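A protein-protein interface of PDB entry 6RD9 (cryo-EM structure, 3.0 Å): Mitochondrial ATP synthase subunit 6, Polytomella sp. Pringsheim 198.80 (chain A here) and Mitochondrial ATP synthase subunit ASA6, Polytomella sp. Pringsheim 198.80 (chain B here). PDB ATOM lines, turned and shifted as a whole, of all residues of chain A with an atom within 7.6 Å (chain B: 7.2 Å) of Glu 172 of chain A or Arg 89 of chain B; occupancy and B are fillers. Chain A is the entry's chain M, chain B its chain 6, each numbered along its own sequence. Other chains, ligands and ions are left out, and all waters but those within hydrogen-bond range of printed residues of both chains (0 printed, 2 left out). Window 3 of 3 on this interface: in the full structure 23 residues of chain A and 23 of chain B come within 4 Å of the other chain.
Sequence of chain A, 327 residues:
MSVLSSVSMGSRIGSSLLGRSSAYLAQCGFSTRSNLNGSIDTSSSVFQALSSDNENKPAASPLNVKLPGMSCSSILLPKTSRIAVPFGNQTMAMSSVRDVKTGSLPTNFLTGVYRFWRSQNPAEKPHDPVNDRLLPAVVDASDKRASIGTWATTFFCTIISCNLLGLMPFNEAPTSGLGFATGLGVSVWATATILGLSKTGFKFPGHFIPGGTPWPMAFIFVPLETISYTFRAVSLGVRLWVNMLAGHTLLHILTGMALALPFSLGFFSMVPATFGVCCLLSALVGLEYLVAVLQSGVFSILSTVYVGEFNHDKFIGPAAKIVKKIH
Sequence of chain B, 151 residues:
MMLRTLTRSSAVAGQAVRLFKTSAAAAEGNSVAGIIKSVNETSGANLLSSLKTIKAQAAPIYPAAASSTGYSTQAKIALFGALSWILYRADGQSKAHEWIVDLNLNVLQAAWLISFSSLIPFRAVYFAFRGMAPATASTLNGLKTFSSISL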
ATOM      1  N   SER A 161      23.614  -7.002   6.442  1.00  0.00           N
ATOM      2  CA  SER A 161      22.468  -7.489   5.696  1.00  0.00           C
ATOM      3  C   SER A 161      22.865  -8.620   4.778  1.00  0.00           C
ATOM      4  O   SER A 161      22.077  -9.529   4.540  1.00  0.00           O
ATOM      5  CB  SER A 161      21.856  -6.366   4.894  1.00  0.00           C
ATOM      6  OG  SER A 161      21.419  -5.354   5.764  1.00  0.00           O
ATOM      7  N   CYS A 162      24.072  -8.569   4.242  1.00  0.00           N
ATOM      8  CA  CYS A 162      24.575  -9.638   3.406  1.00  0.00           C
ATOM      9  C   CYS A 162      25.019 -10.842   4.212  1.00  0.00           C
ATOM     10  O   CYS A 162      24.802 -11.968   3.779  1.00  0.00           O
ATOM     11  CB  CYS A 162      25.735  -9.133   2.566  1.00  0.00           C
ATOM     12  SG  CYS A 162      25.265  -8.103   1.201  1.00  0.00           S
ATOM     13  N   ASN A 163      25.634 -10.635   5.369  1.00  0.00           N
ATOM     14  CA  ASN A 163      26.082 -11.754   6.186  1.00  0.00           C
ATOM     15  C   ASN A 163      24.911 -12.514   6.766  1.00  0.00           C
ATOM     16  O   ASN A 163      24.970 -13.736   6.899  1.00  0.00           O
ATOM     17  CB  ASN A 163      26.963 -11.271   7.322  1.00  0.00           C
ATOM     18  CG  ASN A 163      28.300 -10.838   6.872  1.00  0.00           C
ATOM     19  OD1 ASN A 163      29.052 -10.261   7.635  1.00  0.00           O
ATOM     20  ND2 ASN A 163      28.628 -11.122   5.644  1.00  0.00           N
ATOM     21  N   LEU A 164      23.853 -11.814   7.133  1.00  0.00           N
ATOM     22  CA  LEU A 164      22.694 -12.470   7.696  1.00  0.00           C
ATOM     23  C   LEU A 164      21.790 -13.073   6.647  1.00  0.00           C
ATOM     24  O   LEU A 164      20.877 -13.805   7.015  1.00  0.00           O
ATOM     25  CB  LEU A 164      21.878 -11.506   8.541  1.00  0.00           C
ATOM     26  CG  LEU A 164      22.393 -11.020   9.886  1.00  0.00           C
ATOM     27  CD1 LEU A 164      21.385 -10.073  10.424  1.00  0.00           C
ATOM     28  CD2 LEU A 164      22.626 -12.130  10.847  1.00  0.00           C
ATOM     29  N   LEU A 165      21.981 -12.765   5.367  1.00  0.00           N
ATOM     30  CA  LEU A 165      21.293 -13.536   4.341  1.00  0.00           C
ATOM     31  C   LEU A 165      21.758 -14.969   4.318  1.00  0.00           C
ATOM     32  O   LEU A 165      20.961 -15.856   4.036  1.00  0.00           O
ATOM     33  CB  LEU A 165      21.497 -12.953   2.961  1.00  0.00           C
ATOM     34  CG  LEU A 165      20.654 -11.796   2.530  1.00  0.00           C
ATOM     35  CD1 LEU A 165      21.149 -11.356   1.194  1.00  0.00           C
ATOM     36  CD2 LEU A 165      19.270 -12.320   2.426  1.00  0.00           C
ATOM     37  N   GLY A 166      23.019 -15.223   4.637  1.00  0.00           N
ATOM     38  CA  GLY A 166      23.529 -16.572   4.652  1.00  0.00           C
ATOM     39  C   GLY A 166      22.923 -17.457   5.703  1.00  0.00           C
ATOM     40  O   GLY A 166      23.058 -18.677   5.609  1.00  0.00           O
ATOM     41  N   LEU A 167      22.249 -16.876   6.684  1.00  0.00           N
ATOM     42  CA  LEU A 167      21.581 -17.593   7.750  1.00  0.00           C
ATOM     43  C   LEU A 167      20.080 -17.663   7.558  1.00  0.00           C
ATOM     44  O   LEU A 167      19.395 -18.265   8.377  1.00  0.00           O
ATOM     45  CB  LEU A 167      21.912 -16.932   9.074  1.00  0.00           C
ATOM     46  CG  LEU A 167      23.414 -16.813   9.188  1.00  0.00           C
ATOM     47  CD1 LEU A 167      23.719 -15.749  10.140  1.00  0.00           C
ATOM     48  CD2 LEU A 167      23.949 -18.104   9.690  1.00  0.00           C
ATOM     49  N   MET A 168      19.561 -17.053   6.532  1.00  0.00           N
ATOM     50  CA  MET A 168      18.192 -17.303   6.149  1.00  0.00           C
ATOM     51  C   MET A 168      18.127 -18.582   5.336  1.00  0.00           C
ATOM     52  O   MET A 168      19.067 -18.903   4.615  1.00  0.00           O
ATOM     53  CB  MET A 168      17.640 -16.148   5.332  1.00  0.00           C
ATOM     54  CG  MET A 168      17.583 -14.847   6.065  1.00  0.00           C
ATOM     55  SD  MET A 168      16.717 -14.979   7.622  1.00  0.00           S
ATOM     56  CE  MET A 168      18.025 -14.619   8.779  1.00  0.00           C
ATOM     57  N   PRO A 169      17.057 -19.351   5.465  1.00  0.00           N
ATOM     58  CA  PRO A 169      16.920 -20.551   4.648  1.00  0.00           C
ATOM     59  C   PRO A 169      16.754 -20.215   3.181  1.00  0.00           C
ATOM     60  O   PRO A 169      16.228 -19.166   2.823  1.00  0.00           O
ATOM     61  CB  PRO A 169      15.672 -21.222   5.218  1.00  0.00           C
ATOM     62  CG  PRO A 169      15.027 -20.221   6.018  1.00  0.00           C
ATOM     63  CD  PRO A 169      16.065 -19.334   6.542  1.00  0.00           C
ATOM     64  N   PHE A 170      17.258 -21.117   2.343  1.00  0.00           N
ATOM     65  CA  PHE A 170      17.332 -21.062   0.885  1.00  0.00           C
ATOM     66  C   PHE A 170      18.236 -19.963   0.371  1.00  0.00           C
ATOM     67  O   PHE A 170      18.232 -19.690  -0.823  1.00  0.00           O
ATOM     68  CB  PHE A 170      15.956 -20.925   0.226  1.00  0.00           C
ATOM     69  CG  PHE A 170      14.961 -21.922   0.700  1.00  0.00           C
ATOM     70  CD1 PHE A 170      14.925 -23.186   0.163  1.00  0.00           C
ATOM     71  CD2 PHE A 170      14.055 -21.593   1.677  1.00  0.00           C
ATOM     72  CE1 PHE A 170      14.018 -24.101   0.606  1.00  0.00           C
ATOM     73  CE2 PHE A 170      13.147 -22.504   2.118  1.00  0.00           C
ATOM     74  CZ  PHE A 170      13.128 -23.759   1.578  1.00  0.00           C
ATOM     75  N   ASN A 171      19.040 -19.344   1.218  1.00  0.00           N
ATOM     76  CA  ASN A 171      19.817 -18.191   0.814  1.00  0.00           C
ATOM     77  C   ASN A 171      21.272 -18.383   1.179  1.00  0.00           C
ATOM     78  O   ASN A 171      21.601 -19.077   2.137  1.00  0.00           O
ATOM     79  CB  ASN A 171      19.311 -16.931   1.459  1.00  0.00           C
ATOM     80  CG  ASN A 171      18.151 -16.353   0.747  1.00  0.00           C
ATOM     81  OD1 ASN A 171      18.267 -15.930  -0.385  1.00  0.00           O
ATOM     82  ND2 ASN A 171      17.019 -16.306   1.407  1.00  0.00           N
ATOM     83  N   GLU A 172      22.137 -17.775   0.383  1.00  0.00           N
ATOM     84  CA  GLU A 172      23.552 -17.710   0.668  1.00  0.00           C
ATOM     85  C   GLU A 172      23.933 -16.259   0.861  1.00  0.00           C
ATOM     86  O   GLU A 172      23.249 -15.350   0.398  1.00  0.00           O
ATOM     87  CB  GLU A 172      24.379 -18.330  -0.447  1.00  0.00           C
ATOM     88  CG  GLU A 172      24.336 -17.566  -1.733  1.00  0.00           C
ATOM     89  CD  GLU A 172      24.782 -18.389  -2.913  1.00  0.00           C
ATOM     90  OE1 GLU A 172      24.923 -19.619  -2.759  1.00  0.00           O
ATOM     91  OE2 GLU A 172      24.981 -17.808  -4.000  1.00  0.00           O
ATOM     92  N   ALA A 173      24.995 -16.056   1.578  1.00  0.00           N
ATOM     93  CA  ALA A 173      25.478 -14.720   1.825  1.00  0.00           C
ATOM     94  C   ALA A 173      26.170 -14.207   0.576  1.00  0.00           C
ATOM     95  O   ALA A 173      26.936 -14.946  -0.040  1.00  0.00           O
ATOM     96  CB  ALA A 173      26.436 -14.727   2.993  1.00  0.00           C
ATOM     97  N   PRO A 174      25.900 -12.978   0.147  1.00  0.00           N
ATOM     98  CA  PRO A 174      26.656 -12.430  -0.972  1.00  0.00           C
ATOM     99  C   PRO A 174      28.098 -12.190  -0.633  1.00  0.00           C
ATOM    100  O   PRO A 174      28.948 -12.273  -1.520  1.00  0.00           O
ATOM    101  CB  PRO A 174      25.932 -11.123  -1.265  1.00  0.00           C
ATOM    102  CG  PRO A 174      24.652 -11.281  -0.711  1.00  0.00           C
ATOM    103  CD  PRO A 174      24.776 -12.109   0.483  1.00  0.00           C
ATOM    104  N   THR A 175      28.407 -11.923   0.632  1.00  0.00           N
ATOM    105  CA  THR A 175      29.767 -11.727   1.094  1.00  0.00           C
ATOM    106  C   THR A 175      30.527 -13.024   1.256  1.00  0.00           C
ATOM    107  O   THR A 175      31.636 -13.011   1.769  1.00  0.00           O
ATOM    108  CB  THR A 175      29.772 -10.989   2.417  1.00  0.00           C
ATOM    109  OG1 THR A 175      28.837 -11.612   3.281  1.00  0.00           O
ATOM    110  CG2 THR A 175      29.386  -9.573   2.242  1.00  0.00           C
ATOM    111  N   SER A 176      29.941 -14.144   0.884  1.00  0.00           N
ATOM    112  CA  SER A 176      30.645 -15.396   0.733  1.00  0.00           C
ATOM    113  C   SER A 176      31.234 -15.545  -0.651  1.00  0.00           C
ATOM    114  O   SER A 176      31.815 -16.583  -0.951  1.00  0.00           O
ATOM    115  CB  SER A 176      29.699 -16.548   1.015  1.00  0.00           C
ATOM    116  OG  SER A 176      30.358 -17.772   0.841  1.00  0.00           O
ATOM    117  N   GLY A 177      31.064 -14.551  -1.504  1.00  0.00           N
ATOM    118  CA  GLY A 177      31.706 -14.542  -2.790  1.00  0.00           C
ATOM    119  C   GLY A 177      32.994 -13.757  -2.726  1.00  0.00           C
ATOM    120  O   GLY A 177      33.119 -12.828  -1.964  1.00  0.00           O
ATOM    121  N   HIS A 248      30.489 -21.507   6.543  1.00  0.00           N
ATOM    122  CA  HIS A 248      29.498 -22.214   5.750  1.00  0.00           C
ATOM    123  C   HIS A 248      30.032 -23.535   5.220  1.00  0.00           C
ATOM    124  O   HIS A 248      29.264 -24.473   5.016  1.00  0.00           O
ATOM    125  CB  HIS A 248      29.036 -21.339   4.599  1.00  0.00           C
ATOM    126  CG  HIS A 248      27.848 -21.881   3.878  1.00  0.00           C
ATOM    127  ND1 HIS A 248      26.642 -22.111   4.501  1.00  0.00           N
ATOM    128  CD2 HIS A 248      27.681 -22.242   2.587  1.00  0.00           C
ATOM    129  CE1 HIS A 248      25.782 -22.591   3.623  1.00  0.00           C
ATOM    130  NE2 HIS A 248      26.388 -22.680   2.454  1.00  0.00           N
ATOM    131  N   LEU B  83       8.117 -15.690  -2.646  1.00  0.00           N
ATOM    132  CA  LEU B  83       7.808 -17.077  -2.958  1.00  0.00           C
ATOM    133  C   LEU B  83       8.414 -17.472  -4.287  1.00  0.00           C
ATOM    134  O   LEU B  83       8.828 -18.614  -4.470  1.00  0.00           O
ATOM    135  CB  LEU B  83       6.303 -17.281  -2.986  1.00  0.00           C
ATOM    136  CG  LEU B  83       5.813 -18.711  -3.102  1.00  0.00           C
ATOM    137  CD1 LEU B  83       5.929 -19.404  -1.761  1.00  0.00           C
ATOM    138  CD2 LEU B  83       4.399 -18.728  -3.624  1.00  0.00           C
ATOM    139  N   SER B  84       8.486 -16.538  -5.227  1.00  0.00           N
ATOM    140  CA  SER B  84       9.174 -16.805  -6.479  1.00  0.00           C
ATOM    141  C   SER B  84      10.674 -16.906  -6.289  1.00  0.00           C
ATOM    142  O   SER B  84      11.365 -17.436  -7.156  1.00  0.00           O
ATOM    143  CB  SER B  84       8.860 -15.721  -7.494  1.00  0.00           C
ATOM    144  OG  SER B  84       9.670 -15.869  -8.629  1.00  0.00           O
ATOM    145  N   TRP B  85      11.204 -16.365  -5.198  1.00  0.00           N
ATOM    146  CA  TRP B  85      12.619 -16.505  -4.898  1.00  0.00           C
ATOM    147  C   TRP B  85      12.889 -17.777  -4.125  1.00  0.00           C
ATOM    148  O   TRP B  85      13.889 -18.442  -4.369  1.00  0.00           O
ATOM    149  CB  TRP B  85      13.109 -15.299  -4.108  1.00  0.00           C
ATOM    150  CG  TRP B  85      14.518 -15.377  -3.697  1.00  0.00           C
ATOM    151  CD1 TRP B  85      14.990 -15.655  -2.467  1.00  0.00           C
ATOM    152  CD2 TRP B  85      15.650 -15.149  -4.519  1.00  0.00           C
ATOM    153  NE1 TRP B  85      16.348 -15.633  -2.467  1.00  0.00           N
ATOM    154  CE2 TRP B  85      16.779 -15.323  -3.725  1.00  0.00           C
ATOM    155  CE3 TRP B  85      15.817 -14.821  -5.858  1.00  0.00           C
ATOM    156  CZ2 TRP B  85      18.052 -15.180  -4.222  1.00  0.00           C
ATOM    157  CZ3 TRP B  85      17.077 -14.686  -6.344  1.00  0.00           C
ATOM    158  CH2 TRP B  85      18.177 -14.861  -5.535  1.00  0.00           C
ATOM    159  N   ILE B  86      12.007 -18.135  -3.202  1.00  0.00           N
ATOM    160  CA  ILE B  86      12.231 -19.320  -2.387  1.00  0.00           C
ATOM    161  C   ILE B  86      12.043 -20.578  -3.218  1.00  0.00           C
ATOM    162  O   ILE B  86      12.774 -21.556  -3.059  1.00  0.00           O
ATOM    163  CB  ILE B  86      11.315 -19.272  -1.154  1.00  0.00           C
ATOM    164  CG1 ILE B  86      11.928 -18.356  -0.108  1.00  0.00           C
ATOM    165  CG2 ILE B  86      11.079 -20.631  -0.549  1.00  0.00           C
ATOM    166  CD1 ILE B  86      11.116 -18.221   1.126  1.00  0.00           C
ATOM    167  N   LEU B  87      11.110 -20.554  -4.163  1.00  0.00           N
ATOM    168  CA  LEU B  87      10.954 -21.695  -5.052  1.00  0.00           C
ATOM    169  C   LEU B  87      12.104 -21.799  -6.030  1.00  0.00           C
ATOM    170  O   LEU B  87      12.532 -22.901  -6.352  1.00  0.00           O
ATOM    171  CB  LEU B  87       9.642 -21.604  -5.813  1.00  0.00           C
ATOM    172  CG  LEU B  87       8.419 -21.840  -4.944  1.00  0.00           C
ATOM    173  CD1 LEU B  87       7.183 -21.572  -5.744  1.00  0.00           C
ATOM    174  CD2 LEU B  87       8.426 -23.243  -4.402  1.00  0.00           C
ATOM    175  N   TYR B  88      12.622 -20.681  -6.497  1.00  0.00           N
ATOM    176  CA  TYR B  88      13.723 -20.724  -7.438  1.00  0.00           C
ATOM    177  C   TYR B  88      15.023 -21.099  -6.761  1.00  0.00           C
ATOM    178  O   TYR B  88      15.862 -21.759  -7.368  1.00  0.00           O
ATOM    179  CB  TYR B  88      13.837 -19.375  -8.131  1.00  0.00           C
ATOM    180  CG  TYR B  88      15.184 -19.040  -8.669  1.00  0.00           C
ATOM    181  CD1 TYR B  88      15.648 -19.621  -9.827  1.00  0.00           C
ATOM    182  CD2 TYR B  88      15.986 -18.119  -8.031  1.00  0.00           C
ATOM    183  CE1 TYR B  88      16.877 -19.306 -10.323  1.00  0.00           C
ATOM    184  CE2 TYR B  88      17.216 -17.805  -8.517  1.00  0.00           C
ATOM    185  CZ  TYR B  88      17.654 -18.398  -9.661  1.00  0.00           C
ATOM    186  OH  TYR B  88      18.884 -18.073 -10.149  1.00  0.00           O
ATOM    187  N   ARG B  89      15.209 -20.696  -5.514  1.00  0.00           N
ATOM    188  CA  ARG B  89      16.407 -21.088  -4.802  1.00  0.00           C
ATOM    189  C   ARG B  89      16.341 -22.524  -4.345  1.00  0.00           C
ATOM    190  O   ARG B  89      17.372 -23.183  -4.289  1.00  0.00           O
ATOM    191  CB  ARG B  89      16.625 -20.186  -3.607  1.00  0.00           C
ATOM    192  CG  ARG B  89      17.066 -18.824  -3.959  1.00  0.00           C
ATOM    193  CD  ARG B  89      18.459 -18.805  -4.416  1.00  0.00           C
ATOM    194  NE  ARG B  89      19.318 -19.454  -3.452  1.00  0.00           N
ATOM    195  CZ  ARG B  89      20.626 -19.287  -3.414  1.00  0.00           C
ATOM    196  NH1 ARG B  89      21.212 -18.484  -4.278  1.00  0.00           N
ATOM    197  NH2 ARG B  89      21.345 -19.926  -2.516  1.00  0.00           N
ATOM    198  N   ALA B  90      15.157 -23.029  -4.011  1.00  0.00           N
ATOM    199  CA  ALA B  90      15.011 -24.438  -3.681  1.00  0.00           C
ATOM    200  C   ALA B  90      15.021 -25.320  -4.906  1.00  0.00           C
ATOM    201  O   ALA B  90      15.246 -26.521  -4.782  1.00  0.00           O
ATOM    202  CB  ALA B  90      13.719 -24.687  -2.920  1.00  0.00           C
ATOM    203  N   ASP B  91      14.748 -24.756  -6.074  1.00  0.00           N
ATOM    204  CA  ASP B  91      14.851 -25.517  -7.305  1.00  0.00           C
ATOM    205  C   ASP B  91      16.296 -25.825  -7.627  1.00  0.00           C
ATOM    206  O   ASP B  91      16.653 -26.978  -7.873  1.00  0.00           O
ATOM    207  CB  ASP B  91      14.203 -24.743  -8.443  1.00  0.00           C
ATOM    208  CG  ASP B  91      14.590 -25.267  -9.796  1.00  0.00           C
ATOM    209  OD1 ASP B  91      14.146 -26.375 -10.165  1.00  0.00           O
ATOM    210  OD2 ASP B  91      15.343 -24.565 -10.501  1.00  0.00           O
ATOM    211  N   GLY B  92      17.151 -24.808  -7.610  1.00  0.00           N
ATOM    212  CA  GLY B  92      18.556 -25.003  -7.893  1.00  0.00           C
ATOM    213  C   GLY B  92      19.351 -25.566  -6.748  1.00  0.00           C
ATOM    214  O   GLY B  92      20.503 -25.946  -6.943  1.00  0.00           O
ATOM    215  N   GLN B  93      18.785 -25.578  -5.549  1.00  0.00           N
ATOM    216  CA  GLN B  93      19.394 -26.294  -4.442  1.00  0.00           C
ATOM    217  C   GLN B  93      19.201 -27.780  -4.568  1.00  0.00           C
ATOM    218  O   GLN B  93      20.003 -28.544  -4.035  1.00  0.00           O
ATOM    219  CB  GLN B  93      18.794 -25.872  -3.112  1.00  0.00           C
ATOM    220  CG  GLN B  93      19.509 -24.797  -2.380  1.00  0.00           C
ATOM    221  CD  GLN B  93      18.897 -24.571  -1.044  1.00  0.00           C
ATOM    222  OE1 GLN B  93      17.841 -25.102  -0.744  1.00  0.00           O
ATOM    223  NE2 GLN B  93      19.552 -23.781  -0.223  1.00  0.00           N
ATOM    224  N   SER B  94      18.143 -28.204  -5.233  1.00  0.00           N
ATOM    225  CA  SER B  94      17.822 -29.611  -5.342  1.00  0.00           C
ATOM    226  C   SER B  94      18.557 -30.296  -6.469  1.00  0.00           C
ATOM    227  O   SER B  94      18.402 -31.501  -6.628  1.00  0.00           O
ATOM    228  CB  SER B  94      16.336 -29.774  -5.547  1.00  0.00           C
ATOM    229  OG  SER B  94      15.970 -29.216  -6.787  1.00  0.00           O
ATOM    230  N   LEU B 103      19.583 -29.000   1.100  1.00  0.00           N
ATOM    231  CA  LEU B 103      18.220 -28.952   1.598  1.00  0.00           C
ATOM    232  C   LEU B 103      18.138 -29.244   3.082  1.00  0.00           C
ATOM    233  O   LEU B 103      17.140 -28.895   3.708  1.00  0.00           O
ATOM    234  CB  LEU B 103      17.349 -29.931   0.833  1.00  0.00           C
ATOM    235  CG  LEU B 103      17.086 -29.562  -0.617  1.00  0.00           C
ATOM    236  CD1 LEU B 103      16.531 -30.763  -1.283  1.00  0.00           C
ATOM    237  CD2 LEU B 103      16.150 -28.405  -0.756  1.00  0.00           C
ATOM    238  N   ASN B 106      18.782 -25.706   5.005  1.00  0.00           N
ATOM    239  CA  ASN B 106      17.620 -24.866   5.229  1.00  0.00           C
ATOM    240  C   ASN B 106      16.827 -25.304   6.442  1.00  0.00           C
ATOM    241  O   ASN B 106      16.118 -24.492   7.025  1.00  0.00           O
ATOM    242  CB  ASN B 106      16.721 -24.870   4.009  1.00  0.00           C
ATOM    243  CG  ASN B 106      17.483 -24.730   2.737  1.00  0.00           C
ATOM    244  OD1 ASN B 106      18.552 -24.145   2.709  1.00  0.00           O
ATOM    245  ND2 ASN B 106      16.940 -25.260   1.669  1.00  0.00           N
ATOM    246  N   GLN B 109      19.001 -23.814   9.252  1.00  0.00           N
ATOM    247  CA  GLN B 109      18.915 -22.370   9.318  1.00  0.00           C
ATOM    248  C   GLN B 109      17.555 -21.910   9.798  1.00  0.00           C
ATOM    249  O   GLN B 109      17.473 -20.925  10.529  1.00  0.00           O
ATOM    250  CB  GLN B 109      19.220 -21.777   7.957  1.00  0.00           C
ATOM    251  CG  GLN B 109      20.646 -21.863   7.598  1.00  0.00           C
ATOM    252  CD  GLN B 109      20.861 -21.679   6.142  1.00  0.00           C
ATOM    253  OE1 GLN B 109      19.923 -21.627   5.373  1.00  0.00           O
ATOM    254  NE2 GLN B 109      22.108 -21.570   5.743  1.00  0.00           N
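Of the printed residues of chain B, Glu 172 of chain A touches Arg 89 (3.6 Å).
Of the printed residues of chain A, Ile 86 of chain B touches Phe 170 (3.8 Å).
Of the printed residues of chain A, Ala 90 of chain B touches Phe 170.
Of the printed residues of chain B, Phe 170 of chain A touches Ile 86 (3.8 Å), Arg 89 (2.9 Å), Ala 90 (3.6 Å), Gln 93 (3.6 Å) and Asn 106 (3.3 Å).
The nearest printed residue of chain A that does not touch Ala 90 of chain B is Asn 171 of chain A (7.5 Å).
Leu 167 of chain A touches Gln 109 of chain B.
O of Asn 106 of chain B touches CB of Pro 169 of chain A, 3.8 Å away.
Gln 109 of chain B touches Pro 169 of chain A.
Ile 86 of chain B touches Phe 170 of chain A (CG2 to CD2, 3.8 Å).
Ala 90 of chain B touches Phe 170 of chain A (CB to CE1, 3.6 Å).
Phe 170 of chain A touches Gln 93 of chain B.
Along chain A the printed residues that touch a printed residue of chain B span positions 166 to 172.
Of the 15 printed residues of chain B, 7 touch a printed residue of chain A.
Printed residues of chain B that touch a printed residue of chain A: Trp 85, Ile 86, Arg 89, Ala 90, Gln 93, Asn 106 and Gln 109.
Hydrophobic or aromatic side chains of chain B within 4 Å of the printed part of chain A: Trp 85, Ile 86 and Ala 90.
The backbone carbonyl oxygen of Pro 169 of chain A is in hydrogen-bond range of the side-chain amide nitrogen of Asn 171 of chain A, 3.3 Å away.
O of Ala 90 of chain B lies within hydrogen-bond range of OG of Ser 94 of chain B.
The side-chain amide oxygen of Gln 93 of chain B sits at hydrogen-bond distance from the side-chain amide nitrogen of Asn 106 of chain B, 2.6 Å away.
O of Gly 166 of chain A sits at hydrogen-bond distance from NE2 of Gln 109 of chain B (3.0 Å).
The backbone carbonyl oxygen (O) of Met 168 of chain A lies close to the side-chain amide oxygen (OE1) of Gln 109 of chain B.
The guanidinium group (NE) of Arg 89 of chain B is in hydrogen-bond range of the backbone carbonyl oxygen (O) of Phe 170 of chain A.
The backbone NH of Phe 170 of chain A is in hydrogen-bond range of the side-chain amide oxygen of Asn 106 of chain B (3.3 Å).
OD1 of Asn 171 of chain A lies within hydrogen-bond range of NE1 of Trp 85 of chain B.
The guanidinium group (NH2) of Arg 89 of chain B lies within salt-bridge range of the side-chain carboxylate (OE1) of Glu 172 of chain A, at 3.6 Å.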
